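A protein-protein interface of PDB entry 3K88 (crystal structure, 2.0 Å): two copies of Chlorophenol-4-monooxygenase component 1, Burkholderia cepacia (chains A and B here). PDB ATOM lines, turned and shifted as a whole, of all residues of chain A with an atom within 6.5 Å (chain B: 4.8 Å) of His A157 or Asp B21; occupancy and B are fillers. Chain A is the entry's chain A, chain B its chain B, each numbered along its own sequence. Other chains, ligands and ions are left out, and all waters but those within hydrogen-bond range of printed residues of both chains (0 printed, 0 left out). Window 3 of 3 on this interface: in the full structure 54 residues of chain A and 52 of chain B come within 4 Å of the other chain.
The guanidinium group (NE) of Arg A155 sits at hydrogen-bond distance from a ring nitrogen (NE2) of His A157.
Phe A132 touches Phe B22.
Phe A132 touches Ala B25 (CE1 to CB, 3.5 Å).
NH1 of Arg A155 touches CB of Ala B25, 3.5 Å away.
His A157 touches Asp B21.
Of the 9 printed residues of chain B, 4 touch a printed residue of chain A.
Printed residues of chain B that touch a printed residue of chain A: Asp B21, Phe B22, Asp B24 and Ala B25.
Hydrophobic or aromatic side chains of chain B that line the printed part of chain A: Phe B22 and Ala B25.
Of the 8 printed residues of chain A, 3 touch a printed residue of chain B.
Along chain A the printed residues that touch a printed residue of chain B span positions 132 to 157.
No position is printed for both chains.
Of the 6 pairs that touch across the chains among the printed residues, none has its exchanged pair printed and touching as well.
The side-chain carboxylate (OD1) of Asp B24 is in salt-bridge range of the guanidinium group (NH2) of Arg A155, 3.7 Å away.
The guanidinium group (NH2) of Arg A155 lies within salt-bridge range of the side-chain carboxylate (OD1) of Asp B21, at 2.7 Å.
His A157 touches just one residue of chain B: Asp B21 (3.6 Å).
Of chain A, only Arg A155 (2.7 Å) and His A157 (3.6 Å) come within 4 Å of Asp B21.
Printed residues of chain A within 4 Å of Phe B22: Phe A132 (3.8 Å).
Of the printed residues of chain B, Arg A155 touches Asp B21 (2.7 Å), Asp B24 (3.7 Å) and Ala B25 (3.5 Å).
Of the printed residues of chain A, Ala B25 touches Phe A132 and Arg A155.
Of the printed residues of chain A, Asp B24 touches Arg A155.
Printed residues of chain B within 4 Å of Phe A132: Phe B22 and Ala B25.
The nearest printed residue of chain B that does not touch His A157 is Asp B24 (5.9 Å).
The nearest printed residue of chain A that does not touch Ala B25 is Asn A156 (5.5 Å).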
ATOM      1  N   MET A 126      14.033 -17.187 -12.541  1.00  0.00           N
ATOM      2  CA  MET A 126      13.448 -16.087 -13.372  1.00  0.00           C
ATOM      3  C   MET A 126      11.948 -16.097 -13.625  1.00  0.00           C
ATOM      4  O   MET A 126      11.370 -15.041 -13.940  1.00  0.00           O
ATOM      5  CB  MET A 126      14.153 -15.950 -14.741  1.00  0.00           C
ATOM      6  CG  MET A 126      15.651 -15.749 -14.662  1.00  0.00           C
ATOM      7  SD  MET A 126      16.202 -14.493 -13.468  1.00  0.00           S
ATOM      8  CE  MET A 126      15.433 -13.005 -14.144  1.00  0.00           C
ATOM      9  N   SER A 131      11.465 -12.525  -7.431  1.00  0.00           N
ATOM     10  CA  SER A 131      12.821 -12.965  -7.216  1.00  0.00           C
ATOM     11  C   SER A 131      13.665 -11.771  -6.821  1.00  0.00           C
ATOM     12  O   SER A 131      13.734 -10.762  -7.547  1.00  0.00           O
ATOM     13  CB  SER A 131      13.395 -13.678  -8.431  1.00  0.00           C
ATOM     14  OG  SER A 131      14.722 -14.066  -8.106  1.00  0.00           O
ATOM     15  N   PHE A 132      14.223 -11.842  -5.615  1.00  0.00           N
ATOM     16  CA  PHE A 132      15.051 -10.752  -5.108  1.00  0.00           C
ATOM     17  C   PHE A 132      16.498 -11.221  -5.028  1.00  0.00           C
ATOM     18  O   PHE A 132      16.758 -12.267  -4.468  1.00  0.00           O
ATOM     19  CB  PHE A 132      14.642 -10.369  -3.681  1.00  0.00           C
ATOM     20  CG  PHE A 132      13.473  -9.434  -3.599  1.00  0.00           C
ATOM     21  CD1 PHE A 132      13.024  -8.753  -4.728  1.00  0.00           C
ATOM     22  CD2 PHE A 132      12.861  -9.204  -2.393  1.00  0.00           C
ATOM     23  CE1 PHE A 132      11.942  -7.829  -4.670  1.00  0.00           C
ATOM     24  CE2 PHE A 132      11.782  -8.297  -2.282  1.00  0.00           C
ATOM     25  CZ  PHE A 132      11.326  -7.588  -3.424  1.00  0.00           C
ATOM     26  N   ARG A 155      15.967  -7.347  -8.720  1.00  0.00           N
ATOM     27  CA  ARG A 155      14.682  -8.084  -8.717  1.00  0.00           C
ATOM     28  C   ARG A 155      14.332  -8.653 -10.094  1.00  0.00           C
ATOM     29  O   ARG A 155      14.843  -8.185 -11.113  1.00  0.00           O
ATOM     30  CB  ARG A 155      13.562  -7.255  -8.070  1.00  0.00           C
ATOM     31  CG  ARG A 155      13.165  -5.939  -8.752  1.00  0.00           C
ATOM     32  CD  ARG A 155      11.793  -6.086  -9.448  1.00  0.00           C
ATOM     33  NE  ARG A 155      11.187  -4.803  -9.770  1.00  0.00           N
ATOM     34  CZ  ARG A 155       9.871  -4.603  -9.924  1.00  0.00           C
ATOM     35  NH1 ARG A 155       9.015  -5.618  -9.791  1.00  0.00           N
ATOM     36  NH2 ARG A 155       9.409  -3.380 -10.207  1.00  0.00           N
ATOM     37  N   ASN A 156      13.597  -9.754 -10.179  1.00  0.00           N
ATOM     38  CA  ASN A 156      13.201 -10.134 -11.534  1.00  0.00           C
ATOM     39  C   ASN A 156      12.012  -9.227 -11.893  1.00  0.00           C
ATOM     40  O   ASN A 156      11.104  -9.028 -11.075  1.00  0.00           O
ATOM     41  CB  ASN A 156      12.948 -11.653 -11.724  1.00  0.00           C
ATOM     42  CG  ASN A 156      11.671 -12.177 -10.987  1.00  0.00           C
ATOM     43  OD1 ASN A 156      11.169 -13.315 -11.261  1.00  0.00           O
ATOM     44  ND2 ASN A 156      11.172 -11.377 -10.046  1.00  0.00           N
ATOM     45  N   HIS A 157      12.040  -8.598 -13.066  1.00  0.00           N
ATOM     46  CA  HIS A 157      10.797  -7.981 -13.532  1.00  0.00           C
ATOM     47  C   HIS A 157       9.926  -9.150 -14.060  1.00  0.00           C
ATOM     48  O   HIS A 157      10.129  -9.674 -15.154  1.00  0.00           O
ATOM     49  CB  HIS A 157      11.033  -6.793 -14.478  1.00  0.00           C
ATOM     50  CG  HIS A 157      11.057  -5.452 -13.784  1.00  0.00           C
ATOM     51  ND1 HIS A 157      10.258  -4.388 -14.174  1.00  0.00           N
ATOM     52  CD2 HIS A 157      11.775  -5.001 -12.718  1.00  0.00           C
ATOM     53  CE1 HIS A 157      10.482  -3.346 -13.384  1.00  0.00           C
ATOM     54  NE2 HIS A 157      11.397  -3.688 -12.489  1.00  0.00           N
ATOM     55  N   ALA A 158       8.987  -9.566 -13.205  1.00  0.00           N
ATOM     56  CA  ALA A 158       8.316 -10.868 -13.236  1.00  0.00           C
ATOM     57  C   ALA A 158       7.027 -10.838 -14.065  1.00  0.00           C
ATOM     58  O   ALA A 158       6.282  -9.852 -14.016  1.00  0.00           O
ATOM     59  CB  ALA A 158       7.977 -11.278 -11.758  1.00  0.00           C
ATOM     60  N   GLU A 159       6.747 -11.911 -14.808  1.00  0.00           N
ATOM     61  CA  GLU A 159       5.450 -12.033 -15.501  1.00  0.00           C
ATOM     62  C   GLU A 159       4.414 -12.510 -14.505  1.00  0.00           C
ATOM     63  O   GLU A 159       4.770 -13.070 -13.466  1.00  0.00           O
ATOM     64  CB  GLU A 159       5.509 -13.005 -16.686  1.00  0.00           C
ATOM     65  CG  GLU A 159       6.045 -12.397 -17.985  1.00  0.00           C
ATOM     66  CD  GLU A 159       6.218 -13.445 -19.084  1.00  0.00           C
ATOM     67  OE1 GLU A 159       5.510 -14.479 -19.015  1.00  0.00           O
ATOM     68  OE2 GLU A 159       7.049 -13.240 -20.009  1.00  0.00           O
ATOM     69  N   VAL B  17      17.890  -1.636  -4.778  1.00  0.00           N
ATOM     70  CA  VAL B  17      16.742  -1.269  -5.614  1.00  0.00           C
ATOM     71  C   VAL B  17      15.951  -0.057  -5.046  1.00  0.00           C
ATOM     72  O   VAL B  17      16.022   0.283  -3.846  1.00  0.00           O
ATOM     73  CB  VAL B  17      15.755  -2.462  -5.840  1.00  0.00           C
ATOM     74  CG1 VAL B  17      16.462  -3.607  -6.522  1.00  0.00           C
ATOM     75  CG2 VAL B  17      15.078  -2.905  -4.506  1.00  0.00           C
ATOM     76  N   ALA B  18      15.210   0.585  -5.933  1.00  0.00           N
ATOM     77  CA  ALA B  18      14.340   1.705  -5.579  1.00  0.00           C
ATOM     78  C   ALA B  18      13.306   1.171  -4.588  1.00  0.00           C
ATOM     79  O   ALA B  18      12.868   0.029  -4.734  1.00  0.00           O
ATOM     80  CB  ALA B  18      13.615   2.244  -6.889  1.00  0.00           C
ATOM     81  N   SER B  19      12.956   1.955  -3.570  1.00  0.00           N
ATOM     82  CA  SER B  19      11.850   1.629  -2.661  1.00  0.00           C
ATOM     83  C   SER B  19      10.541   1.347  -3.439  1.00  0.00           C
ATOM     84  O   SER B  19       9.775   0.427  -3.058  1.00  0.00           O
ATOM     85  CB  SER B  19      11.561   2.806  -1.699  1.00  0.00           C
ATOM     86  OG  SER B  19      12.718   3.016  -0.914  1.00  0.00           O
ATOM     87  N   PHE B  20      10.243   2.170  -4.462  1.00  0.00           N
ATOM     88  CA  PHE B  20       9.096   1.879  -5.353  1.00  0.00           C
ATOM     89  C   PHE B  20       9.139   0.463  -5.949  1.00  0.00           C
ATOM     90  O   PHE B  20       8.148  -0.252  -5.969  1.00  0.00           O
ATOM     91  CB  PHE B  20       9.007   2.860  -6.531  1.00  0.00           C
ATOM     92  CG  PHE B  20       7.840   2.537  -7.456  1.00  0.00           C
ATOM     93  CD1 PHE B  20       6.585   3.026  -7.193  1.00  0.00           C
ATOM     94  CD2 PHE B  20       8.010   1.686  -8.536  1.00  0.00           C
ATOM     95  CE1 PHE B  20       5.481   2.646  -7.990  1.00  0.00           C
ATOM     96  CE2 PHE B  20       6.933   1.319  -9.358  1.00  0.00           C
ATOM     97  CZ  PHE B  20       5.655   1.807  -9.069  1.00  0.00           C
ATOM     98  N   ASP B  21      10.275   0.065  -6.489  1.00  0.00           N
ATOM     99  CA  ASP B  21      10.412  -1.301  -7.062  1.00  0.00           C
ATOM    100  C   ASP B  21      10.299  -2.416  -6.021  1.00  0.00           C
ATOM    101  O   ASP B  21       9.720  -3.454  -6.273  1.00  0.00           O
ATOM    102  CB  ASP B  21      11.768  -1.443  -7.753  1.00  0.00           C
ATOM    103  CG  ASP B  21      11.774  -0.894  -9.188  1.00  0.00           C
ATOM    104  OD1 ASP B  21      10.804  -1.123  -9.968  1.00  0.00           O
ATOM    105  OD2 ASP B  21      12.781  -0.258  -9.527  1.00  0.00           O
ATOM    106  N   PHE B  22      10.903  -2.217  -4.856  1.00  0.00           N
ATOM    107  CA  PHE B  22      10.784  -3.186  -3.721  1.00  0.00           C
ATOM    108  C   PHE B  22       9.273  -3.438  -3.410  1.00  0.00           C
ATOM    109  O   PHE B  22       8.810  -4.561  -3.407  1.00  0.00           O
ATOM    110  CB  PHE B  22      11.489  -2.569  -2.524  1.00  0.00           C
ATOM    111  CG  PHE B  22      11.418  -3.382  -1.258  1.00  0.00           C
ATOM    112  CD1 PHE B  22      10.571  -3.006  -0.221  1.00  0.00           C
ATOM    113  CD2 PHE B  22      12.161  -4.563  -1.118  1.00  0.00           C
ATOM    114  CE1 PHE B  22      10.516  -3.777   0.962  1.00  0.00           C
ATOM    115  CE2 PHE B  22      12.102  -5.307   0.076  1.00  0.00           C
ATOM    116  CZ  PHE B  22      11.316  -4.900   1.090  1.00  0.00           C
ATOM    117  N   ARG B  23       8.504  -2.383  -3.200  1.00  0.00           N
ATOM    118  CA  ARG B  23       7.056  -2.508  -2.900  1.00  0.00           C
ATOM    119  C   ARG B  23       6.242  -3.107  -4.040  1.00  0.00           C
ATOM    120  O   ARG B  23       5.381  -3.974  -3.834  1.00  0.00           O
ATOM    121  CB  ARG B  23       6.420  -1.117  -2.569  1.00  0.00           C
ATOM    122  CG  ARG B  23       6.942  -0.484  -1.283  1.00  0.00           C
ATOM    123  CD  ARG B  23       6.097   0.735  -0.864  1.00  0.00           C
ATOM    124  NE  ARG B  23       5.893   1.671  -1.958  1.00  0.00           N
ATOM    125  CZ  ARG B  23       6.691   2.709  -2.225  1.00  0.00           C
ATOM    126  NH1 ARG B  23       7.789   2.950  -1.506  1.00  0.00           N
ATOM    127  NH2 ARG B  23       6.393   3.515  -3.235  1.00  0.00           N
ATOM    128  N   ASP B  24       6.485  -2.634  -5.255  1.00  0.00           N
ATOM    129  CA  ASP B  24       5.774  -3.225  -6.392  1.00  0.00           C
ATOM    130  C   ASP B  24       6.021  -4.718  -6.545  1.00  0.00           C
ATOM    131  O   ASP B  24       5.077  -5.515  -6.748  1.00  0.00           O
ATOM    132  CB  ASP B  24       6.127  -2.530  -7.708  1.00  0.00           C
ATOM    133  CG  ASP B  24       5.202  -2.978  -8.803  1.00  0.00           C
ATOM    134  OD1 ASP B  24       5.672  -3.279  -9.927  1.00  0.00           O
ATOM    135  OD2 ASP B  24       3.988  -3.083  -8.474  1.00  0.00           O
ATOM    136  N   ALA B  25       7.295  -5.119  -6.472  1.00  0.00           N
ATOM    137  CA  ALA B  25       7.623  -6.546  -6.568  1.00  0.00           C
ATOM    138  C   ALA B  25       6.912  -7.332  -5.459  1.00  0.00           C
ATOM    139  O   ALA B  25       6.317  -8.344  -5.736  1.00  0.00           O
ATOM    140  CB  ALA B  25       9.141  -6.777  -6.487  1.00  0.00           C
